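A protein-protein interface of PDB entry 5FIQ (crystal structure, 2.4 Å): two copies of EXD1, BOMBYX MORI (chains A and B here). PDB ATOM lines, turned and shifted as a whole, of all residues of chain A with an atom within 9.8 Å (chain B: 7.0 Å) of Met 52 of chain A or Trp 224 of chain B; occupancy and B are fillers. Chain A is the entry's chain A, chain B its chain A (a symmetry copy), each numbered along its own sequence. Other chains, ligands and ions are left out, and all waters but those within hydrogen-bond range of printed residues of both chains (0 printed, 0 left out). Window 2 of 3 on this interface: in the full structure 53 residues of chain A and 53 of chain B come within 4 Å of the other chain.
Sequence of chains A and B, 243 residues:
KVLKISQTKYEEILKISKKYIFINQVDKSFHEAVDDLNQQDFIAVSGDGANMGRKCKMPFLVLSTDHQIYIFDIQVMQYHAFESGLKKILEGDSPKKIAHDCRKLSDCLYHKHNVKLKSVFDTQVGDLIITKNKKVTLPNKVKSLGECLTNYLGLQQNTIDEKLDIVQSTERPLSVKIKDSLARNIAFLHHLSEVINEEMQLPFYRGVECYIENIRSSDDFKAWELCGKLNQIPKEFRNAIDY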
ATOM      1  N   GLY A  47       8.437 -19.399 -11.327  1.00  0.00           N
ATOM      2  CA  GLY A  47       9.779 -18.817 -11.453  1.00  0.00           C
ATOM      3  C   GLY A  47      10.987 -19.768 -11.143  1.00  0.00           C
ATOM      4  O   GLY A  47      12.137 -19.439 -11.466  1.00  0.00           O
ATOM      5  N   ASP A  48      10.697 -20.914 -10.540  1.00  0.00           N
ATOM      6  CA  ASP A  48      11.755 -21.872 -10.150  1.00  0.00           C
ATOM      7  C   ASP A  48      12.513 -22.295 -11.361  1.00  0.00           C
ATOM      8  O   ASP A  48      11.919 -22.727 -12.344  1.00  0.00           O
ATOM      9  CB  ASP A  48      11.192 -23.131  -9.413  1.00  0.00           C
ATOM     10  CG  ASP A  48      10.769 -22.830  -7.966  1.00  0.00           C
ATOM     11  OD1 ASP A  48      11.239 -21.814  -7.462  1.00  0.00           O
ATOM     12  OD2 ASP A  48       9.866 -23.495  -7.367  1.00  0.00           O
ATOM     13  N   GLY A  49      13.840 -22.195 -11.294  1.00  0.00           N
ATOM     14  CA  GLY A  49      14.699 -22.551 -12.432  1.00  0.00           C
ATOM     15  C   GLY A  49      15.294 -21.393 -13.205  1.00  0.00           C
ATOM     16  O   GLY A  49      16.099 -21.636 -14.037  1.00  0.00           O
ATOM     17  N   ALA A  50      14.769 -20.174 -13.033  1.00  0.00           N
ATOM     18  CA  ALA A  50      15.247 -19.003 -13.743  1.00  0.00           C
ATOM     19  C   ALA A  50      15.649 -17.928 -12.785  1.00  0.00           C
ATOM     20  O   ALA A  50      15.576 -16.751 -13.075  1.00  0.00           O
ATOM     21  CB  ALA A  50      14.171 -18.485 -14.649  1.00  0.00           C
ATOM     22  N   ASN A  51      16.201 -18.336 -11.657  1.00  0.00           N
ATOM     23  CA  ASN A  51      16.641 -17.408 -10.623  1.00  0.00           C
ATOM     24  C   ASN A  51      17.857 -16.604 -10.938  1.00  0.00           C
ATOM     25  O   ASN A  51      18.121 -15.667 -10.208  1.00  0.00           O
ATOM     26  CB  ASN A  51      16.932 -18.166  -9.336  1.00  0.00           C
ATOM     27  CG  ASN A  51      15.724 -18.914  -8.871  1.00  0.00           C
ATOM     28  OD1 ASN A  51      14.639 -18.331  -8.635  1.00  0.00           O
ATOM     29  ND2 ASN A  51      15.859 -20.233  -8.827  1.00  0.00           N
ATOM     30  N   MET A  52      18.531 -16.892 -12.045  1.00  0.00           N
ATOM     31  CA  MET A  52      19.686 -16.135 -12.440  1.00  0.00           C
ATOM     32  C   MET A  52      19.430 -15.264 -13.652  1.00  0.00           C
ATOM     33  O   MET A  52      20.320 -14.582 -14.146  1.00  0.00           O
ATOM     34  CB  MET A  52      20.781 -17.127 -12.759  1.00  0.00           C
ATOM     35  CG  MET A  52      21.168 -18.109 -11.587  1.00  0.00           C
ATOM     36  SD  MET A  52      22.915 -17.992 -11.187  1.00  0.00           S
ATOM     37  CE  MET A  52      23.201 -16.251 -10.863  1.00  0.00           C
ATOM     38  N   GLY A  53      18.184 -15.248 -14.098  1.00  0.00           N
ATOM     39  CA  GLY A  53      17.804 -14.529 -15.273  1.00  0.00           C
ATOM     40  C   GLY A  53      18.620 -15.026 -16.444  1.00  0.00           C
ATOM     41  O   GLY A  53      18.797 -16.249 -16.607  1.00  0.00           O
ATOM     42  N   ARG A  54      19.092 -14.054 -17.252  1.00  0.00           N
ATOM     43  CA  ARG A  54      19.860 -14.362 -18.448  1.00  0.00           C
ATOM     44  C   ARG A  54      21.175 -15.053 -18.150  1.00  0.00           C
ATOM     45  O   ARG A  54      21.641 -15.809 -18.986  1.00  0.00           O
ATOM     46  CB  ARG A  54      20.105 -13.119 -19.325  1.00  0.00           C
ATOM     47  CG  ARG A  54      20.933 -12.032 -18.673  1.00  0.00           C
ATOM     48  CD  ARG A  54      21.045 -10.802 -19.542  1.00  0.00           C
ATOM     49  NE  ARG A  54      19.790 -10.114 -19.682  1.00  0.00           N
ATOM     50  CZ  ARG A  54      19.645  -8.862 -20.097  1.00  0.00           C
ATOM     51  NH1 ARG A  54      20.700  -8.113 -20.366  1.00  0.00           N
ATOM     52  NH2 ARG A  54      18.417  -8.333 -20.230  1.00  0.00           N
ATOM     53  N   LYS A  55      21.717 -14.906 -16.947  1.00  0.00           N
ATOM     54  CA  LYS A  55      23.008 -15.504 -16.634  1.00  0.00           C
ATOM     55  C   LYS A  55      23.005 -17.016 -16.818  1.00  0.00           C
ATOM     56  O   LYS A  55      24.083 -17.630 -16.898  1.00  0.00           O
ATOM     57  CB  LYS A  55      23.457 -15.140 -15.217  1.00  0.00           C
ATOM     58  CG  LYS A  55      23.793 -13.683 -14.992  1.00  0.00           C
ATOM     59  CD  LYS A  55      25.094 -13.276 -15.684  1.00  0.00           C
ATOM     60  CE  LYS A  55      25.434 -11.774 -15.573  1.00  0.00           C
ATOM     61  NZ  LYS A  55      25.746 -11.434 -14.138  1.00  0.00           N
ATOM     62  N   CYS A  56      21.840 -17.660 -16.844  1.00  0.00           N
ATOM     63  CA  CYS A  56      21.808 -19.115 -16.695  1.00  0.00           C
ATOM     64  C   CYS A  56      20.608 -19.828 -17.245  1.00  0.00           C
ATOM     65  O   CYS A  56      19.489 -19.403 -16.991  1.00  0.00           O
ATOM     66  CB  CYS A  56      21.860 -19.419 -15.205  1.00  0.00           C
ATOM     67  SG  CYS A  56      22.774 -20.915 -14.996  1.00  0.00           S
ATOM     68  N   LYS A  57      20.827 -20.909 -17.966  1.00  0.00           N
ATOM     69  CA  LYS A  57      19.774 -21.726 -18.468  1.00  0.00           C
ATOM     70  C   LYS A  57      18.897 -22.308 -17.347  1.00  0.00           C
ATOM     71  O   LYS A  57      19.270 -22.379 -16.172  1.00  0.00           O
ATOM     72  CB  LYS A  57      20.286 -22.883 -19.289  1.00  0.00           C
ATOM     73  CG  LYS A  57      20.632 -22.585 -20.737  1.00  0.00           C
ATOM     74  CD  LYS A  57      21.286 -23.821 -21.412  1.00  0.00           C
ATOM     75  CE  LYS A  57      20.362 -24.535 -22.428  1.00  0.00           C
ATOM     76  NZ  LYS A  57      20.489 -23.865 -23.755  1.00  0.00           N
ATOM     77  N   MET A  58      17.706 -22.746 -17.759  1.00  0.00           N
ATOM     78  CA  MET A  58      16.728 -23.323 -16.906  1.00  0.00           C
ATOM     79  C   MET A  58      17.063 -24.816 -16.895  1.00  0.00           C
ATOM     80  O   MET A  58      17.128 -25.450 -17.944  1.00  0.00           O
ATOM     81  CB  MET A  58      15.275 -23.107 -17.405  1.00  0.00           C
ATOM     82  CG  MET A  58      14.810 -21.669 -17.268  1.00  0.00           C
ATOM     83  SD  MET A  58      13.040 -21.449 -17.451  1.00  0.00           S
ATOM     84  CE  MET A  58      12.410 -21.839 -15.793  1.00  0.00           C
ATOM     85  N   PRO A  59      17.184 -25.383 -15.713  1.00  0.00           N
ATOM     86  CA  PRO A  59      17.298 -26.836 -15.650  1.00  0.00           C
ATOM     87  C   PRO A  59      15.940 -27.540 -15.695  1.00  0.00           C
ATOM     88  O   PRO A  59      15.858 -28.721 -16.143  1.00  0.00           O
ATOM     89  CB  PRO A  59      17.962 -27.082 -14.288  1.00  0.00           C
ATOM     90  CG  PRO A  59      17.473 -25.899 -13.438  1.00  0.00           C
ATOM     91  CD  PRO A  59      17.273 -24.747 -14.386  1.00  0.00           C
ATOM     92  N   ARG A 103       9.668 -11.267 -13.561  1.00  0.00           N
ATOM     93  CA  ARG A 103      10.783 -10.473 -14.159  1.00  0.00           C
ATOM     94  C   ARG A 103      11.987 -11.336 -14.554  1.00  0.00           C
ATOM     95  O   ARG A 103      12.401 -11.336 -15.675  1.00  0.00           O
ATOM     96  CB  ARG A 103      11.317  -9.370 -13.245  1.00  0.00           C
ATOM     97  CG  ARG A 103      10.423  -8.143 -13.083  1.00  0.00           C
ATOM     98  CD  ARG A 103      10.139  -7.951 -11.611  1.00  0.00           C
ATOM     99  NE  ARG A 103      10.646  -6.809 -10.878  1.00  0.00           N
ATOM    100  CZ  ARG A 103      10.650  -6.749  -9.530  1.00  0.00           C
ATOM    101  NH1 ARG A 103      10.241  -7.762  -8.770  1.00  0.00           N
ATOM    102  NH2 ARG A 103      11.094  -5.658  -8.909  1.00  0.00           N
ATOM    103  N   LYS A 104      12.526 -12.116 -13.644  1.00  0.00           N
ATOM    104  CA  LYS A 104      13.715 -12.970 -13.953  1.00  0.00           C
ATOM    105  C   LYS A 104      13.380 -14.017 -14.957  1.00  0.00           C
ATOM    106  O   LYS A 104      14.150 -14.342 -15.813  1.00  0.00           O
ATOM    107  CB  LYS A 104      14.232 -13.600 -12.702  1.00  0.00           C
ATOM    108  CG  LYS A 104      14.960 -12.646 -11.804  1.00  0.00           C
ATOM    109  CD  LYS A 104      15.258 -13.339 -10.461  1.00  0.00           C
ATOM    110  CE  LYS A 104      16.542 -12.827  -9.888  1.00  0.00           C
ATOM    111  NZ  LYS A 104      16.992 -13.699  -8.724  1.00  0.00           N
ATOM    112  N   LEU A 105      12.162 -14.479 -14.894  1.00  0.00           N
ATOM    113  CA  LEU A 105      11.696 -15.514 -15.820  1.00  0.00           C
ATOM    114  C   LEU A 105      11.589 -15.042 -17.248  1.00  0.00           C
ATOM    115  O   LEU A 105      11.978 -15.795 -18.142  1.00  0.00           O
ATOM    116  CB  LEU A 105      10.372 -16.134 -15.334  1.00  0.00           C
ATOM    117  CG  LEU A 105       9.728 -17.156 -16.266  1.00  0.00           C
ATOM    118  CD1 LEU A 105      10.466 -18.465 -16.378  1.00  0.00           C
ATOM    119  CD2 LEU A 105       8.295 -17.389 -15.878  1.00  0.00           C
ATOM    120  N   SER A 106      11.027 -13.813 -17.447  1.00  0.00           N
ATOM    121  CA  SER A 106      10.981 -13.165 -18.744  1.00  0.00           C
ATOM    122  C   SER A 106      12.382 -13.076 -19.269  1.00  0.00           C
ATOM    123  O   SER A 106      12.670 -13.537 -20.363  1.00  0.00           O
ATOM    124  CB  SER A 106      10.358 -11.747 -18.658  1.00  0.00           C
ATOM    125  OG  SER A 106      10.213 -11.160 -19.947  1.00  0.00           O
ATOM    126  N   ASP A 107      13.273 -12.536 -18.450  1.00  0.00           N
ATOM    127  CA  ASP A 107      14.679 -12.383 -18.823  1.00  0.00           C
ATOM    128  C   ASP A 107      15.359 -13.717 -19.247  1.00  0.00           C
ATOM    129  O   ASP A 107      16.030 -13.781 -20.282  1.00  0.00           O
ATOM    130  CB  ASP A 107      15.469 -11.815 -17.633  1.00  0.00           C
ATOM    131  CG  ASP A 107      16.877 -11.282 -18.045  1.00  0.00           C
ATOM    132  OD1 ASP A 107      17.083 -10.915 -19.195  1.00  0.00           O
ATOM    133  OD2 ASP A 107      17.798 -11.253 -17.193  1.00  0.00           O
ATOM    134  N   CYS A 108      15.180 -14.773 -18.438  1.00  0.00           N
ATOM    135  CA  CYS A 108      15.816 -16.013 -18.695  1.00  0.00           C
ATOM    136  C   CYS A 108      15.346 -16.715 -19.933  1.00  0.00           C
ATOM    137  O   CYS A 108      16.120 -17.131 -20.793  1.00  0.00           O
ATOM    138  CB  CYS A 108      15.620 -16.944 -17.481  1.00  0.00           C
ATOM    139  SG  CYS A 108      16.384 -18.557 -17.699  1.00  0.00           S
ATOM    140  N   LEU A 109      14.062 -16.852 -20.032  1.00  0.00           N
ATOM    141  CA  LEU A 109      13.420 -17.392 -21.257  1.00  0.00           C
ATOM    142  C   LEU A 109      13.806 -16.714 -22.588  1.00  0.00           C
ATOM    143  O   LEU A 109      13.956 -17.394 -23.630  1.00  0.00           O
ATOM    144  CB  LEU A 109      11.944 -17.305 -21.120  1.00  0.00           C
ATOM    145  CG  LEU A 109      11.270 -18.306 -20.218  1.00  0.00           C
ATOM    146  CD1 LEU A 109       9.826 -17.872 -19.930  1.00  0.00           C
ATOM    147  CD2 LEU A 109      11.232 -19.660 -20.859  1.00  0.00           C
ATOM    148  N   HIS A 111      16.686 -14.592 -23.328  1.00  0.00           N
ATOM    149  CA  HIS A 111      18.107 -14.658 -23.646  1.00  0.00           C
ATOM    150  C   HIS A 111      18.737 -16.076 -23.636  1.00  0.00           C
ATOM    151  O   HIS A 111      19.768 -16.274 -24.266  1.00  0.00           O
ATOM    152  CB  HIS A 111      18.857 -13.719 -22.726  1.00  0.00           C
ATOM    153  CG  HIS A 111      18.547 -12.267 -22.974  1.00  0.00           C
ATOM    154  ND1 HIS A 111      17.703 -11.527 -22.163  1.00  0.00           N
ATOM    155  CD2 HIS A 111      18.938 -11.417 -23.959  1.00  0.00           C
ATOM    156  CE1 HIS A 111      17.600 -10.288 -22.620  1.00  0.00           C
ATOM    157  NE2 HIS A 111      18.317 -10.200 -23.722  1.00  0.00           N
ATOM    158  N   LYS A 112      18.132 -17.042 -22.965  1.00  0.00           N
ATOM    159  CA  LYS A 112      18.690 -18.377 -22.958  1.00  0.00           C
ATOM    160  C   LYS A 112      17.912 -19.409 -23.637  1.00  0.00           C
ATOM    161  O   LYS A 112      18.420 -20.493 -23.917  1.00  0.00           O
ATOM    162  CB  LYS A 112      18.909 -18.902 -21.495  1.00  0.00           C
ATOM    163  CG  LYS A 112      19.782 -18.014 -20.635  1.00  0.00           C
ATOM    164  CD  LYS A 112      21.157 -17.758 -21.257  1.00  0.00           C
ATOM    165  CE  LYS A 112      22.137 -18.746 -20.722  1.00  0.00           C
ATOM    166  NZ  LYS A 112      23.395 -18.403 -21.390  1.00  0.00           N
ATOM    167  N   LEU A 164      16.196 -23.408  -3.543  1.00  0.00           N
ATOM    168  CA  LEU A 164      16.486 -24.685  -4.122  1.00  0.00           C
ATOM    169  C   LEU A 164      17.987 -24.751  -4.374  1.00  0.00           C
ATOM    170  O   LEU A 164      18.626 -23.755  -4.739  1.00  0.00           O
ATOM    171  CB  LEU A 164      15.709 -24.916  -5.407  1.00  0.00           C
ATOM    172  CG  LEU A 164      14.213 -25.177  -5.174  1.00  0.00           C
ATOM    173  CD1 LEU A 164      13.603 -25.517  -6.499  1.00  0.00           C
ATOM    174  CD2 LEU A 164      13.905 -26.321  -4.221  1.00  0.00           C
ATOM    175  N   ILE A 166      21.183 -25.287  -5.913  1.00  0.00           N
ATOM    176  CA  ILE A 166      21.594 -24.996  -7.297  1.00  0.00           C
ATOM    177  C   ILE A 166      22.305 -26.213  -7.909  1.00  0.00           C
ATOM    178  O   ILE A 166      22.127 -26.512  -9.064  1.00  0.00           O
ATOM    179  CB  ILE A 166      22.528 -23.744  -7.408  1.00  0.00           C
ATOM    180  CG1 ILE A 166      22.005 -22.527  -6.563  1.00  0.00           C
ATOM    181  CG2 ILE A 166      22.689 -23.311  -8.859  1.00  0.00           C
ATOM    182  CD1 ILE A 166      20.507 -22.237  -6.618  1.00  0.00           C
ATOM    183  N   THR A 170      20.914 -29.260 -10.990  1.00  0.00           N
ATOM    184  CA  THR A 170      21.560 -29.662 -12.257  1.00  0.00           C
ATOM    185  C   THR A 170      21.972 -31.133 -12.292  1.00  0.00           C
ATOM    186  O   THR A 170      22.364 -31.625 -13.339  1.00  0.00           O
ATOM    187  CB  THR A 170      22.769 -28.763 -12.610  1.00  0.00           C
ATOM    188  OG1 THR A 170      23.546 -28.526 -11.440  1.00  0.00           O
ATOM    189  CG2 THR A 170      22.316 -27.423 -13.122  1.00  0.00           C
ATOM    190  N   ILE B 215      13.479  -6.437 -16.860  1.00  0.00           N
ATOM    191  CA  ILE B 215      14.809  -7.044 -16.906  1.00  0.00           C
ATOM    192  C   ILE B 215      15.162  -7.454 -18.346  1.00  0.00           C
ATOM    193  O   ILE B 215      16.268  -7.193 -18.823  1.00  0.00           O
ATOM    194  CB  ILE B 215      14.922  -8.220 -15.864  1.00  0.00           C
ATOM    195  CG1 ILE B 215      14.552  -7.678 -14.497  1.00  0.00           C
ATOM    196  CG2 ILE B 215      16.290  -8.822 -15.873  1.00  0.00           C
ATOM    197  CD1 ILE B 215      14.862  -8.557 -13.346  1.00  0.00           C
ATOM    198  N   SER B 218      16.737  -4.792 -20.524  1.00  0.00           N
ATOM    199  CA  SER B 218      17.954  -4.097 -20.037  1.00  0.00           C
ATOM    200  C   SER B 218      19.194  -4.720 -20.660  1.00  0.00           C
ATOM    201  O   SER B 218      19.160  -5.862 -21.065  1.00  0.00           O
ATOM    202  CB  SER B 218      18.025  -4.169 -18.508  1.00  0.00           C
ATOM    203  OG  SER B 218      16.954  -3.457 -17.890  1.00  0.00           O
ATOM    204  N   ASP B 219      20.270  -3.965 -20.735  1.00  0.00           N
ATOM    205  CA  ASP B 219      21.576  -4.522 -21.075  1.00  0.00           C
ATOM    206  C   ASP B 219      22.111  -5.346 -19.876  1.00  0.00           C
ATOM    207  O   ASP B 219      21.573  -5.288 -18.734  1.00  0.00           O
ATOM    208  CB  ASP B 219      22.601  -3.466 -21.498  1.00  0.00           C
ATOM    209  CG  ASP B 219      22.924  -2.437 -20.403  1.00  0.00           C
ATOM    210  OD1 ASP B 219      22.971  -2.720 -19.185  1.00  0.00           O
ATOM    211  OD2 ASP B 219      23.214  -1.290 -20.780  1.00  0.00           O
ATOM    212  N   ASP B 220      23.138  -6.123 -20.151  1.00  0.00           N
ATOM    213  CA  ASP B 220      23.614  -7.100 -19.164  1.00  0.00           C
ATOM    214  C   ASP B 220      23.925  -6.524 -17.801  1.00  0.00           C
ATOM    215  O   ASP B 220      23.572  -7.106 -16.782  1.00  0.00           O
ATOM    216  CB  ASP B 220      24.804  -7.857 -19.722  1.00  0.00           C
ATOM    217  CG  ASP B 220      24.414  -8.815 -20.823  1.00  0.00           C
ATOM    218  OD1 ASP B 220      23.254  -9.207 -20.889  1.00  0.00           O
ATOM    219  OD2 ASP B 220      25.254  -9.228 -21.596  1.00  0.00           O
ATOM    220  N   PHE B 221      24.519  -5.350 -17.766  1.00  0.00           N
ATOM    221  CA  PHE B 221      24.906  -4.814 -16.487  1.00  0.00           C
ATOM    222  C   PHE B 221      23.665  -4.513 -15.651  1.00  0.00           C
ATOM    223  O   PHE B 221      23.553  -4.948 -14.533  1.00  0.00           O
ATOM    224  CB  PHE B 221      25.841  -3.611 -16.620  1.00  0.00           C
ATOM    225  CG  PHE B 221      26.261  -3.040 -15.294  1.00  0.00           C
ATOM    226  CD1 PHE B 221      27.172  -3.700 -14.476  1.00  0.00           C
ATOM    227  CD2 PHE B 221      25.691  -1.864 -14.820  1.00  0.00           C
ATOM    228  CE1 PHE B 221      27.538  -3.179 -13.227  1.00  0.00           C
ATOM    229  CE2 PHE B 221      26.056  -1.340 -13.583  1.00  0.00           C
ATOM    230  CZ  PHE B 221      26.972  -2.003 -12.782  1.00  0.00           C
ATOM    231  N   LYS B 222      22.752  -3.762 -16.197  1.00  0.00           N
ATOM    232  CA  LYS B 222      21.569  -3.321 -15.458  1.00  0.00           C
ATOM    233  C   LYS B 222      20.665  -4.500 -15.120  1.00  0.00           C
ATOM    234  O   LYS B 222      19.979  -4.474 -14.119  1.00  0.00           O
ATOM    235  CB  LYS B 222      20.795  -2.248 -16.272  1.00  0.00           C
ATOM    236  CG  LYS B 222      19.704  -1.540 -15.468  1.00  0.00           C
ATOM    237  CD  LYS B 222      18.881  -0.559 -16.315  1.00  0.00           C
ATOM    238  CE  LYS B 222      17.431  -0.451 -15.825  1.00  0.00           C
ATOM    239  NZ  LYS B 222      16.577   0.229 -16.839  1.00  0.00           N
ATOM    240  N   ALA B 223      20.714  -5.516 -15.978  1.00  0.00           N
ATOM    241  CA  ALA B 223      20.009  -6.749 -15.768  1.00  0.00           C
ATOM    242  C   ALA B 223      20.455  -7.421 -14.469  1.00  0.00           C
ATOM    243  O   ALA B 223      19.610  -7.819 -13.659  1.00  0.00           O
ATOM    244  CB  ALA B 223      20.224  -7.703 -16.925  1.00  0.00           C
ATOM    245  N   TRP B 224      21.776  -7.555 -14.309  1.00  0.00           N
ATOM    246  CA  TRP B 224      22.333  -8.120 -13.145  1.00  0.00           C
ATOM    247  C   TRP B 224      21.974  -7.340 -11.901  1.00  0.00           C
ATOM    248  O   TRP B 224      21.390  -7.885 -10.987  1.00  0.00           O
ATOM    249  CB  TRP B 224      23.834  -8.251 -13.314  1.00  0.00           C
ATOM    250  CG  TRP B 224      24.480  -8.979 -12.218  1.00  0.00           C
ATOM    251  CD1 TRP B 224      25.601  -8.611 -11.557  1.00  0.00           C
ATOM    252  CD2 TRP B 224      24.065 -10.264 -11.685  1.00  0.00           C
ATOM    253  NE1 TRP B 224      25.910  -9.562 -10.630  1.00  0.00           N
ATOM    254  CE2 TRP B 224      25.002 -10.596 -10.684  1.00  0.00           C
ATOM    255  CE3 TRP B 224      22.982 -11.159 -11.951  1.00  0.00           C
ATOM    256  CZ2 TRP B 224      24.929 -11.820  -9.937  1.00  0.00           C
ATOM    257  CZ3 TRP B 224      22.885 -12.374 -11.205  1.00  0.00           C
ATOM    258  CH2 TRP B 224      23.875 -12.690 -10.213  1.00  0.00           C
ATOM    259  N   GLU B 225      22.263  -6.055 -11.897  1.00  0.00           N
ATOM    260  CA  GLU B 225      21.841  -5.178 -10.796  1.00  0.00           C
ATOM    261  C   GLU B 225      20.400  -5.379 -10.353  1.00  0.00           C
ATOM    262  O   GLU B 225      20.116  -5.334  -9.166  1.00  0.00           O
ATOM    263  CB  GLU B 225      21.887  -3.705 -11.214  1.00  0.00           C
ATOM    264  CG  GLU B 225      23.154  -2.951 -10.972  1.00  0.00           C
ATOM    265  CD  GLU B 225      22.958  -1.457 -11.221  1.00  0.00           C
ATOM    266  OE1 GLU B 225      21.862  -0.963 -11.011  1.00  0.00           O
ATOM    267  OE2 GLU B 225      23.933  -0.771 -11.603  1.00  0.00           O
ATOM    268  N   LEU B 226      19.491  -5.444 -11.326  1.00  0.00           N
ATOM    269  CA  LEU B 226      18.058  -5.471 -11.062  1.00  0.00           C
ATOM    270  C   LEU B 226      17.693  -6.765 -10.430  1.00  0.00           C
ATOM    271  O   LEU B 226      16.802  -6.773  -9.616  1.00  0.00           O
ATOM    272  CB  LEU B 226      17.243  -5.255 -12.330  1.00  0.00           C
ATOM    273  CG  LEU B 226      17.062  -3.801 -12.852  1.00  0.00           C
ATOM    274  CD1 LEU B 226      16.370  -3.876 -14.194  1.00  0.00           C
ATOM    275  CD2 LEU B 226      16.277  -2.870 -11.933  1.00  0.00           C
ATOM    276  N   CYS B 227      18.402  -7.841 -10.774  1.00  0.00           N
ATOM    277  CA  CYS B 227      18.239  -9.145 -10.086  1.00  0.00           C
ATOM    278  C   CYS B 227      18.635  -9.137  -8.613  1.00  0.00           C
ATOM    279  O   CYS B 227      18.147  -9.947  -7.859  1.00  0.00           O
ATOM    280  CB  CYS B 227      18.990 -10.282 -10.819  1.00  0.00           C
ATOM    281  SG  CYS B 227      18.371 -10.565 -12.497  1.00  0.00           S
ATOM    282  N   GLY B 228      19.542  -8.259  -8.210  1.00  0.00           N
ATOM    283  CA  GLY B 228      19.882  -8.066  -6.792  1.00  0.00           C
ATOM    284  C   GLY B 228      18.825  -7.312  -6.002  1.00  0.00           C
ATOM    285  O   GLY B 228      18.654  -7.555  -4.820  1.00  0.00           O
ATOM    286  N   LYS B 229      18.075  -6.447  -6.671  1.00  0.00           N
ATOM    287  CA  LYS B 229      17.097  -5.533  -6.049  1.00  0.00           C
ATOM    288  C   LYS B 229      15.632  -5.908  -6.293  1.00  0.00           C
ATOM    289  O   LYS B 229      14.774  -5.037  -6.386  1.00  0.00           O
ATOM    290  CB  LYS B 229      17.338  -4.107  -6.600  1.00  0.00           C
ATOM    291  CG  LYS B 229      18.280  -3.263  -5.734  1.00  0.00           C
ATOM    292  CD  LYS B 229      19.234  -2.390  -6.543  1.00  0.00           C
ATOM    293  CE  LYS B 229      18.474  -1.253  -7.222  1.00  0.00           C
ATOM    294  NZ  LYS B 229      19.433  -0.303  -7.830  1.00  0.00           N
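Among the printed residues, pairs that only touch across the chains: Asp 107 of chain A with Ile 215 of chain B, Lys 55 of chain A with Trp 224 of chain B, Arg 54 of chain A with Ala 223 of chain B, Arg 103 of chain A with Ile 215 of chain B, Lys 104 of chain A with Cys 227 of chain B and Met 52 of chain A with Trp 224 of chain B.
No position is printed for both chains.
Of the printed residues of chain B, Met 52 of chain A touches Trp 224 (3.7 Å). Trp 224 of chain B touches two residues of chain A. Of chain A, only Arg 54 (3.4 Å) comes within 4 Å of Ala 223 of chain B. Of the printed residues of chain A, Asp 219 of chain B touches Arg 54 (3.1 Å). Of the printed residues of chain B, Arg 54 of chain A touches Ile 215 (2.8 Å), Ser 218 (2.7 Å), Asp 219 (3.1 Å), Asp 220 (2.8 Å) and Ala 223 (3.4 Å). Ser 106 of chain A touches none of the printed residues of chain B. Lys 229 of chain B touches none of the printed residues of chain A. The nearest residue of chain B that does not touch Met 52 of chain A is Cys 227 of chain B (4.8 Å). The nearest residue of chain A that does not touch Trp 224 of chain B is Asn 51 of chain A (5.9 Å). The nearest printed residue of chain A that does not touch Ile 215 of chain B is Lys 104 of chain A (4.3 Å).
The side-chain carboxylate (OD1) of Asp 219 of chain B is in hydrogen-bond range of the backbone NH (N) of Lys 222 of chain B, at 3.2 Å. The side-chain carboxylate (OD1) of Asp 219 of chain B sits close to the backbone NH (N) of Phe 221 of chain B, 3.4 Å away. OD1 of Asp 107 of chain A lies within hydrogen-bond range of ND1 of His 111 of chain A, 3.1 Å away. The backbone carbonyl oxygen (O) of Asn 51 of chain A sits at hydrogen-bond distance from the side-chain amino group (NZ) of Lys 104 of chain A. The backbone carbonyl oxygen (O) of Ala 223 of chain B is in hydrogen-bond range of the side-chain sulfur (SG) of Cys 227 of chain B (3.2 Å). The guanidinium group of Arg 54 of chain A lies within salt-bridge range of the side-chain carboxylate of Asp 107 of chain A (2.9 Å).
Hydrophobic or aromatic side chains of chain A that line the printed part of chain B: Met 52. Of the 13 printed residues of chain B, 7 touch a printed residue of chain A. Hydrophobic or aromatic side chains of chain B that line the printed part of chain A: Ile 215, Ala 223 and Trp 224. Among the printed residues, 10 pairs touch across the chains. Among the printed residues, Asp or Glu carboxylates within 4 Å of a Lys or Arg side-chain nitrogen of the other chain: Arg 54 of chain A with Asp 220 of chain B.
O of Ile 215 of chain B is in hydrogen-bond range of NH2 of Arg 54 of chain A (2.8 Å). NH1 of Arg 54 of chain A sits close to O of Asp 219 of chain B, 3.4 Å away. The guanidinium group (NH2) of Arg 54 of chain A is in hydrogen-bond range of the backbone carbonyl oxygen (O) of Ser 218 of chain B (2.7 Å). The side-chain carboxylate of Asp 220 of chain B lies within salt-bridge range of the guanidinium group of Arg 54 of chain A (2.8 Å).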
